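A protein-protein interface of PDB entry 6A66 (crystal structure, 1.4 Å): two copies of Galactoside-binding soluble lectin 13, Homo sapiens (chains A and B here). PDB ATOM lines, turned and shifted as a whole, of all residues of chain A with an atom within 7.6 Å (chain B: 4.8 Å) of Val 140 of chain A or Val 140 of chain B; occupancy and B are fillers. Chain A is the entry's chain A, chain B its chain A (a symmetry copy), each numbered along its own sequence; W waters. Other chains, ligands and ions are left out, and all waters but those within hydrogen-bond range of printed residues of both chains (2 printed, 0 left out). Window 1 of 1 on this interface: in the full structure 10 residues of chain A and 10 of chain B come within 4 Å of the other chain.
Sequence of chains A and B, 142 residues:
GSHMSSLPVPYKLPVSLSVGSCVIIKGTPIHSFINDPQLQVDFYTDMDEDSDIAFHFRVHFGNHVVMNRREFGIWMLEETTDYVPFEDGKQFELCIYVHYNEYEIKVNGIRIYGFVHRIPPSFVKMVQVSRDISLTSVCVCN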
ATOM      1  N   LEU A  13     -13.547  24.623  -9.833  1.00  0.00           N
ATOM      2  CA  LEU A  13     -13.699  24.631  -8.375  1.00  0.00           C
ATOM      3  C   LEU A  13     -13.050  23.404  -7.770  1.00  0.00           C
ATOM      4  O   LEU A  13     -13.535  22.293  -7.999  1.00  0.00           O
ATOM      5  CB  LEU A  13     -15.192  24.648  -8.044  1.00  0.00           C
ATOM      6  CG  LEU A  13     -15.580  24.547  -6.570  1.00  0.00           C
ATOM      7  CD1 LEU A  13     -15.136  25.804  -5.833  1.00  0.00           C
ATOM      8  CD2 LEU A  13     -17.075  24.351  -6.480  1.00  0.00           C
ATOM      9  N   PRO A  14     -11.991  23.539  -6.980  1.00  0.00           N
ATOM     10  CA  PRO A  14     -11.487  22.386  -6.233  1.00  0.00           C
ATOM     11  C   PRO A  14     -12.573  21.907  -5.281  1.00  0.00           C
ATOM     12  O   PRO A  14     -13.267  22.707  -4.654  1.00  0.00           O
ATOM     13  CB  PRO A  14     -10.280  22.964  -5.469  1.00  0.00           C
ATOM     14  CG  PRO A  14      -9.947  24.248  -6.191  1.00  0.00           C
ATOM     15  CD  PRO A  14     -11.262  24.776  -6.640  1.00  0.00           C
ATOM     16  N   VAL A  15     -12.734  20.583  -5.186  1.00  0.00           N
ATOM     17  CA  VAL A  15     -13.788  19.985  -4.372  1.00  0.00           C
ATOM     18  C   VAL A  15     -13.269  18.717  -3.697  1.00  0.00           C
ATOM     19  O   VAL A  15     -12.251  18.145  -4.095  1.00  0.00           O
ATOM     20  CB  VAL A  15     -15.084  19.625  -5.154  1.00  0.00           C
ATOM     21  CG1 VAL A  15     -15.692  20.884  -5.775  1.00  0.00           C
ATOM     22  CG2 VAL A  15     -14.811  18.533  -6.209  1.00  0.00           C
ATOM     23  N   SER A  16     -13.947  18.336  -2.623  1.00  0.00           N
ATOM     24  CA  SER A  16     -13.856  16.999  -2.053  1.00  0.00           C
ATOM     25  C   SER A  16     -15.289  16.509  -1.959  1.00  0.00           C
ATOM     26  O   SER A  16     -16.130  17.162  -1.329  1.00  0.00           O
ATOM     27  CB  SER A  16     -13.207  17.027  -0.674  1.00  0.00           C
ATOM     28  OG  SER A  16     -13.360  15.762  -0.053  1.00  0.00           O
ATOM     29  N   LEU A  17     -15.581  15.405  -2.633  1.00  0.00           N
ATOM     30  CA  LEU A  17     -16.926  14.877  -2.665  1.00  0.00           C
ATOM     31  C   LEU A  17     -16.983  13.561  -1.903  1.00  0.00           C
ATOM     32  O   LEU A  17     -16.033  12.770  -1.903  1.00  0.00           O
ATOM     33  CB  LEU A  17     -17.405  14.602  -4.101  1.00  0.00           C
ATOM     34  CG  LEU A  17     -17.489  15.784  -5.063  1.00  0.00           C
ATOM     35  CD1 LEU A  17     -18.028  15.333  -6.435  1.00  0.00           C
ATOM     36  CD2 LEU A  17     -18.348  16.885  -4.499  1.00  0.00           C
ATOM     37  N   SER A  18     -18.110  13.331  -1.258  1.00  0.00           N
ATOM     38  CA  SER A  18     -18.370  12.063  -0.619  1.00  0.00           C
ATOM     39  C   SER A  18     -19.831  11.735  -0.849  1.00  0.00           C
ATOM     40  O   SER A  18     -20.605  12.528  -1.391  1.00  0.00           O
ATOM     41  CB  SER A  18     -18.033  12.106   0.871  1.00  0.00           C
ATOM     42  OG  SER A  18     -18.853  13.033   1.531  1.00  0.00           O
ATOM     43  N   SER A  21     -22.813  14.386  -0.618  1.00  0.00           N
ATOM     44  CA  SER A  21     -22.522  15.712  -1.141  1.00  0.00           C
ATOM     45  C   SER A  21     -23.519  16.109  -2.229  1.00  0.00           C
ATOM     46  O   SER A  21     -24.049  15.264  -2.948  1.00  0.00           O
ATOM     47  CB  SER A  21     -21.131  15.733  -1.780  1.00  0.00           C
ATOM     48  OG  SER A  21     -20.114  15.521  -0.843  1.00  0.00           O
ATOM     49  N   CYS A  22     -23.801  17.398  -2.316  1.00  0.00           N
ATOM     50  CA  CYS A  22     -24.593  17.941  -3.410  1.00  0.00           C
ATOM     51  C   CYS A  22     -23.861  19.135  -3.998  1.00  0.00           C
ATOM     52  O   CYS A  22     -23.398  20.007  -3.261  1.00  0.00           O
ATOM     53  CB  CYS A  22     -25.977  18.402  -2.940  1.00  0.00           C
ATOM     54  SG  CYS A  22     -27.128  18.822  -4.288  1.00  0.00           S
ATOM     55  N   VAL A  23     -23.750  19.172  -5.325  1.00  0.00           N
ATOM     56  CA  VAL A  23     -23.210  20.315  -6.046  1.00  0.00           C
ATOM     57  C   VAL A  23     -24.393  21.059  -6.639  1.00  0.00           C
ATOM     58  O   VAL A  23     -25.193  20.477  -7.386  1.00  0.00           O
ATOM     59  CB  VAL A  23     -22.227  19.859  -7.132  1.00  0.00           C
ATOM     60  CG1 VAL A  23     -21.736  21.055  -7.927  1.00  0.00           C
ATOM     61  CG2 VAL A  23     -21.064  19.079  -6.537  1.00  0.00           C
ATOM     62  N   ILE A  24     -24.505  22.341  -6.321  1.00  0.00           N
ATOM     63  CA  ILE A  24     -25.635  23.166  -6.737  1.00  0.00           C
ATOM     64  C   ILE A  24     -25.074  24.299  -7.575  1.00  0.00           C
ATOM     65  O   ILE A  24     -24.234  25.070  -7.108  1.00  0.00           O
ATOM     66  CB  ILE A  24     -26.416  23.719  -5.532  1.00  0.00           C
ATOM     67  CG1 ILE A  24     -26.852  22.584  -4.630  1.00  0.00           C
ATOM     68  CG2 ILE A  24     -27.652  24.509  -5.983  1.00  0.00           C
ATOM     69  CD1 ILE A  24     -25.870  22.280  -3.522  1.00  0.00           C
ATOM     70  N   ILE A  25     -25.534  24.382  -8.823  1.00  0.00           N
ATOM     71  CA  ILE A  25     -25.066  25.342  -9.815  1.00  0.00           C
ATOM     72  C   ILE A  25     -26.276  26.156 -10.256  1.00  0.00           C
ATOM     73  O   ILE A  25     -27.280  25.588 -10.704  1.00  0.00           O
ATOM     74  CB  ILE A  25     -24.431  24.616 -11.003  1.00  0.00           C
ATOM     75  CG1 ILE A  25     -23.161  23.869 -10.587  1.00  0.00           C
ATOM     76  CG2 ILE A  25     -24.094  25.579 -12.112  1.00  0.00           C
ATOM     77  CD1 ILE A  25     -22.830  22.651 -11.473  1.00  0.00           C
ATOM     78  N   VAL A 127     -14.487  20.345  -9.978  1.00  0.00           N
ATOM     79  CA  VAL A 127     -15.679  20.459 -10.801  1.00  0.00           C
ATOM     80  C   VAL A 127     -15.508  21.643 -11.704  1.00  0.00           C
ATOM     81  O   VAL A 127     -15.231  22.751 -11.244  1.00  0.00           O
ATOM     82  CB  VAL A 127     -16.941  20.640  -9.954  1.00  0.00           C
ATOM     83  CG1 VAL A 127     -18.147  20.871 -10.816  1.00  0.00           C
ATOM     84  CG2 VAL A 127     -17.134  19.390  -9.115  1.00  0.00           C
ATOM     85  N   VAL A 138     -22.131  28.726  -7.250  1.00  0.00           N
ATOM     86  CA  VAL A 138     -21.870  27.299  -7.177  1.00  0.00           C
ATOM     87  C   VAL A 138     -21.642  26.962  -5.711  1.00  0.00           C
ATOM     88  O   VAL A 138     -20.825  27.612  -5.047  1.00  0.00           O
ATOM     89  CB  VAL A 138     -20.619  26.889  -7.973  1.00  0.00           C
ATOM     90  CG1 VAL A 138     -20.351  25.418  -7.829  1.00  0.00           C
ATOM     91  CG2 VAL A 138     -20.826  27.236  -9.438  1.00  0.00           C
ATOM     92  N   CYS A 139     -22.344  25.965  -5.214  1.00  0.00           N
ATOM     93  CA  CYS A 139     -22.239  25.541  -3.822  1.00  0.00           C
ATOM     94  C   CYS A 139     -22.002  24.040  -3.762  1.00  0.00           C
ATOM     95  O   CYS A 139     -22.523  23.263  -4.573  1.00  0.00           O
ATOM     96  CB  CYS A 139     -23.532  25.811  -3.063  1.00  0.00           C
ATOM     97  SG  CYS A 139     -23.914  27.513  -2.770  1.00  0.00           S
ATOM     98  N   VAL A 140     -21.241  23.627  -2.749  1.00  0.00           N
ATOM     99  CA  VAL A 140     -21.033  22.222  -2.433  1.00  0.00           C
ATOM    100  C   VAL A 140     -21.484  22.020  -0.991  1.00  0.00           C
ATOM    101  O   VAL A 140     -20.931  22.623  -0.065  1.00  0.00           O
ATOM    102  CB  VAL A 140     -19.571  21.800  -2.633  1.00  0.00           C
ATOM    103  CG1 VAL A 140     -19.393  20.331  -2.296  1.00  0.00           C
ATOM    104  CG2 VAL A 140     -19.160  22.091  -4.078  1.00  0.00           C
ATOM    105  N   CYS A 141     -22.486  21.189  -0.805  1.00  0.00           N
ATOM    106  CA  CYS A 141     -23.130  21.002   0.482  1.00  0.00           C
ATOM    107  C   CYS A 141     -23.066  19.547   0.931  1.00  0.00           C
ATOM    108  O   CYS A 141     -22.945  18.624   0.119  1.00  0.00           O
ATOM    109  CB  CYS A 141     -24.617  21.405   0.401  1.00  0.00           C
ATOM    110  SG  CYS A 141     -24.929  23.145   0.109  1.00  0.00           S
ATOM    111  N   ASN A 142     -23.161  19.349   2.249  1.00  0.00           N
ATOM    112  CA  ASN A 142     -23.305  18.022   2.851  1.00  0.00           C
ATOM    113  C   ASN A 142     -24.311  18.106   4.005  1.00  0.00           C
ATOM    114  O   ASN A 142     -24.654  19.209   4.444  1.00  0.00           O
ATOM    115  CB  ASN A 142     -21.973  17.512   3.402  1.00  0.00           C
ATOM    116  CG  ASN A 142     -20.960  17.247   2.309  1.00  0.00           C
ATOM    117  OD1 ASN A 142     -20.798  16.109   1.861  1.00  0.00           O
ATOM    118  ND2 ASN A 142     -20.266  18.292   1.879  1.00  0.00           N
ATOM    119  N   LEU B  13     -14.190  18.800   7.132  1.00  0.00           N
ATOM    120  CA  LEU B  13     -14.542  18.983   5.720  1.00  0.00           C
ATOM    121  C   LEU B  13     -13.353  19.511   4.945  1.00  0.00           C
ATOM    122  O   LEU B  13     -12.938  20.649   5.180  1.00  0.00           O
ATOM    123  CB  LEU B  13     -15.702  19.977   5.636  1.00  0.00           C
ATOM    124  CG  LEU B  13     -16.157  20.399   4.240  1.00  0.00           C
ATOM    125  CD1 LEU B  13     -16.779  19.209   3.520  1.00  0.00           C
ATOM    126  CD2 LEU B  13     -17.139  21.538   4.380  1.00  0.00           C
ATOM    127  N   VAL B  15     -11.674  21.573   2.176  1.00  0.00           N
ATOM    128  CA  VAL B  15     -12.184  22.766   1.507  1.00  0.00           C
ATOM    129  C   VAL B  15     -11.074  23.413   0.681  1.00  0.00           C
ATOM    130  O   VAL B  15      -9.886  23.146   0.874  1.00  0.00           O
ATOM    131  CB  VAL B  15     -12.771  23.843   2.464  1.00  0.00           C
ATOM    132  CG1 VAL B  15     -13.949  23.264   3.250  1.00  0.00           C
ATOM    133  CG2 VAL B  15     -11.681  24.416   3.392  1.00  0.00           C
ATOM    134  N   SER B  16     -11.493  24.212  -0.291  1.00  0.00           N
ATOM    135  CA  SER B  16     -10.636  25.188  -0.949  1.00  0.00           C
ATOM    136  C   SER B  16     -11.378  26.507  -0.841  1.00  0.00           C
ATOM    137  O   SER B  16     -12.528  26.612  -1.287  1.00  0.00           O
ATOM    138  CB  SER B  16     -10.400  24.823  -2.410  1.00  0.00           C
ATOM    139  OG  SER B  16      -9.777  25.910  -3.075  1.00  0.00           O
ATOM    140  N   LEU B  17     -10.756  27.485  -0.198  1.00  0.00           N
ATOM    141  CA  LEU B  17     -11.389  28.766   0.018  1.00  0.00           C
ATOM    142  C   LEU B  17     -10.684  29.836  -0.805  1.00  0.00           C
ATOM    143  O   LEU B  17      -9.465  29.801  -1.006  1.00  0.00           O
ATOM    144  CB  LEU B  17     -11.328  29.200   1.492  1.00  0.00           C
ATOM    145  CG  LEU B  17     -12.015  28.312   2.526  1.00  0.00           C
ATOM    146  CD1 LEU B  17     -11.892  28.921   3.936  1.00  0.00           C
ATOM    147  CD2 LEU B  17     -13.463  28.089   2.176  1.00  0.00           C
ATOM    148  N   CYS B  22     -18.154  31.438   0.934  1.00  0.00           N
ATOM    149  CA  CYS B  22     -18.917  31.487   2.173  1.00  0.00           C
ATOM    150  C   CYS B  22     -19.074  30.074   2.707  1.00  0.00           C
ATOM    151  O   CYS B  22     -19.428  29.161   1.960  1.00  0.00           O
ATOM    152  CB  CYS B  22     -20.313  32.085   1.960  1.00  0.00           C
ATOM    153  SG  CYS B  22     -21.218  32.448   3.499  1.00  0.00           S
ATOM    154  N   VAL B  23     -18.803  29.892   3.999  1.00  0.00           N
ATOM    155  CA  VAL B  23     -19.045  28.636   4.692  1.00  0.00           C
ATOM    156  C   VAL B  23     -20.310  28.823   5.512  1.00  0.00           C
ATOM    157  O   VAL B  23     -20.392  29.741   6.340  1.00  0.00           O
ATOM    158  CB  VAL B  23     -17.849  28.262   5.576  1.00  0.00           C
ATOM    159  CG1 VAL B  23     -18.150  26.993   6.353  1.00  0.00           C
ATOM    160  CG2 VAL B  23     -16.576  28.115   4.755  1.00  0.00           C
ATOM    161  N   VAL B 138     -23.613  21.553   6.220  1.00  0.00           N
ATOM    162  CA  VAL B 138     -22.491  22.453   6.018  1.00  0.00           C
ATOM    163  C   VAL B 138     -22.337  22.645   4.516  1.00  0.00           C
ATOM    164  O   VAL B 138     -22.274  21.659   3.771  1.00  0.00           O
ATOM    165  CB  VAL B 138     -21.174  21.885   6.576  1.00  0.00           C
ATOM    166  CG1 VAL B 138     -20.029  22.819   6.301  1.00  0.00           C
ATOM    167  CG2 VAL B 138     -21.319  21.673   8.073  1.00  0.00           C
ATOM    168  N   CYS B 139     -22.274  23.885   4.078  1.00  0.00           N
ATOM    169  CA  CYS B 139     -22.141  24.218   2.665  1.00  0.00           C
ATOM    170  C   CYS B 139     -20.986  25.189   2.475  1.00  0.00           C
ATOM    171  O   CYS B 139     -20.724  26.065   3.311  1.00  0.00           O
ATOM    172  CB  CYS B 139     -23.390  24.916   2.142  1.00  0.00           C
ATOM    173  SG  CYS B 139     -24.840  23.912   2.019  1.00  0.00           S
ATOM    174  N   VAL B 140     -20.318  25.058   1.330  1.00  0.00           N
ATOM    175  CA  VAL B 140     -19.289  25.992   0.899  1.00  0.00           C
ATOM    176  C   VAL B 140     -19.717  26.530  -0.461  1.00  0.00           C
ATOM    177  O   VAL B 140     -19.859  25.769  -1.426  1.00  0.00           O
ATOM    178  CB  VAL B 140     -17.905  25.331   0.836  1.00  0.00           C
ATOM    179  CG1 VAL B 140     -16.859  26.334   0.385  1.00  0.00           C
ATOM    180  CG2 VAL B 140     -17.563  24.753   2.211  1.00  0.00           C
ATOM    181  N   CYS B 141     -19.935  27.824  -0.534  1.00  0.00           N
ATOM    182  CA  CYS B 141     -20.490  28.468  -1.709  1.00  0.00           C
ATOM    183  C   CYS B 141     -19.556  29.543  -2.251  1.00  0.00           C
ATOM    184  O   CYS B 141     -18.727  30.104  -1.527  1.00  0.00           O
ATOM    185  CB  CYS B 141     -21.835  29.143  -1.366  1.00  0.00           C
ATOM    186  SG  CYS B 141     -23.165  28.029  -0.922  1.00  0.00           S
ATOM    187  N   ASN B 142     -19.707  29.834  -3.547  1.00  0.00           N
ATOM    188  CA  ASN B 142     -19.032  30.960  -4.197  1.00  0.00           C
ATOM    189  C   ASN B 142     -20.012  31.632  -5.167  1.00  0.00           C
ATOM    190  O   ASN B 142     -21.063  31.059  -5.477  1.00  0.00           O
ATOM    191  CB  ASN B 142     -17.807  30.496  -4.986  1.00  0.00           C
ATOM    192  CG  ASN B 142     -16.714  29.959  -4.089  1.00  0.00           C
ATOM    193  OD1 ASN B 142     -15.771  30.677  -3.742  1.00  0.00           O
ATOM    194  ND2 ASN B 142     -16.825  28.693  -3.712  1.00  0.00           N
HETATM  195  O   HOH W   1     -18.401  27.114  -5.259  1.00  0.00           O
HETATM  196  O   HOH W   2     -20.132  20.419   3.559  1.00  0.00           O
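The backbone carbonyl oxygen (O) of Val 138 of chain A lies within hydrogen-bond range of the backbone NH (N) of Asn 142 of chain B, 2.9 Å away.
The side-chain sulfur of Cys 141 of chain B is disulfide-bonded to the side-chain sulfur of Cys 139 of chain A, 2.1 Å away.
O of Val 140 of chain B lies within hydrogen-bond range of N of Val 140 of chain A, 2.9 Å away.
The side-chain sulfur of Cys 141 of chain A forms a disulfide with the side-chain sulfur of Cys 139 of chain B, at 2.1 Å.
The backbone NH (N) of Asn 142 of chain A sits at hydrogen-bond distance from the backbone carbonyl oxygen (O) of Val 138 of chain B (2.9 Å).
The backbone carbonyl oxygen of Val 127 of chain A lies within hydrogen-bond range of the backbone NH of Leu 13 of chain A (2.9 Å).
The side-chain hydroxyl (OG) of Ser 21 of chain A sits at hydrogen-bond distance from the side-chain amide oxygen (OD1) of Asn 142 of chain A, 2.9 Å away.
The backbone NH of Cys 22 of chain A is in hydrogen-bond range of the backbone carbonyl oxygen of Cys 141 of chain A, 2.9 Å away.
The backbone NH of Ile 24 of chain A sits at hydrogen-bond distance from the backbone carbonyl oxygen of Cys 139 of chain A (2.8 Å).
The backbone NH (N) of Cys 22 of chain B sits at hydrogen-bond distance from the backbone carbonyl oxygen (O) of Cys 141 of chain B, at 2.9 Å.
Among the printed residues, pairs that only touch across the chains: Leu 13 of chain A with Asn 142 of chain B (3.96 Å), Pro 14 of chain A with Ser 16 of chain B (3.5 Å), Val 138 of chain A with Cys 141 of chain B (3.5 Å), Cys 139 of chain A with Val 140 of chain B (3.4 Å), Val 140 of chain A with Cys 139 of chain B (3.4 Å), Cys 141 of chain A with Val 138 of chain B (3.5 Å) and Asn 142 of chain A with Leu 13 of chain B (3.96 Å).
Val 140 of chain A touches just these residues of chain B: Cys 139 and Val 140.
Val 140 of chain B touches just these residues of chain A: Cys 139 (3.4 Å) and Val 140 (2.9 Å).
Of the printed residues of chain B, Pro 14 of chain A touches Ser 16.
Of the printed residues of chain B, Asn 142 of chain A touches Leu 13 (3.96 Å) and Val 138 (2.9 Å).
Of the printed residues of chain B, Cys 141 of chain A touches Val 138 and Cys 139.
Printed residues of chain A within 4 Å of Cys 141 of chain B: Val 138 (3.5 Å) and Cys 139 (2.1 Å).
Of the printed residues of chain B, Leu 13 of chain A touches Asn 142 (3.96 Å).
The nearest residue of chain A that does not touch Val 140 of chain B is Val 138 of chain A (4.2 Å).
Hydrophobic or aromatic side chains of chain B that line the printed part of chain A: Leu 13.
Of the 17 printed residues of chain A, 7 touch a printed residue of chain B.
Hydrophobic or aromatic side chains of chain A within 4 Å of the printed part of chain B: Leu 13 and Pro 14.
Val 138 of chain A touches Cys 141 of chain B, and with the chains exchanged Cys 141 of chain A touches Val 138 of chain B.
Val 138 of chain A touches Asn 142 of chain B, and with the chains exchanged Asn 142 of chain A touches Val 138 of chain B.
Cys 139 of chain A touches Cys 141 of chain B, and with the chains exchanged Cys 141 of chain A touches Cys 139 of chain B.
Val 140 of chain A touches its own counterpart, Val 140 of chain B.
Of the 12 pairs that touch across the chains among the printed residues, 11 have their exchanged pair printed and touching as well.
Water W1 bridges the backbone carbonyl oxygen of Val 138 of chain A and the side-chain amide nitrogen of Asn 142 of chain B.
Water W2 lies within hydrogen-bond range of the backbone carbonyl oxygen of Val 138 of chain B (2.5 Å) and the side-chain amide nitrogen of Asn 142 of chain A (2.7 Å).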
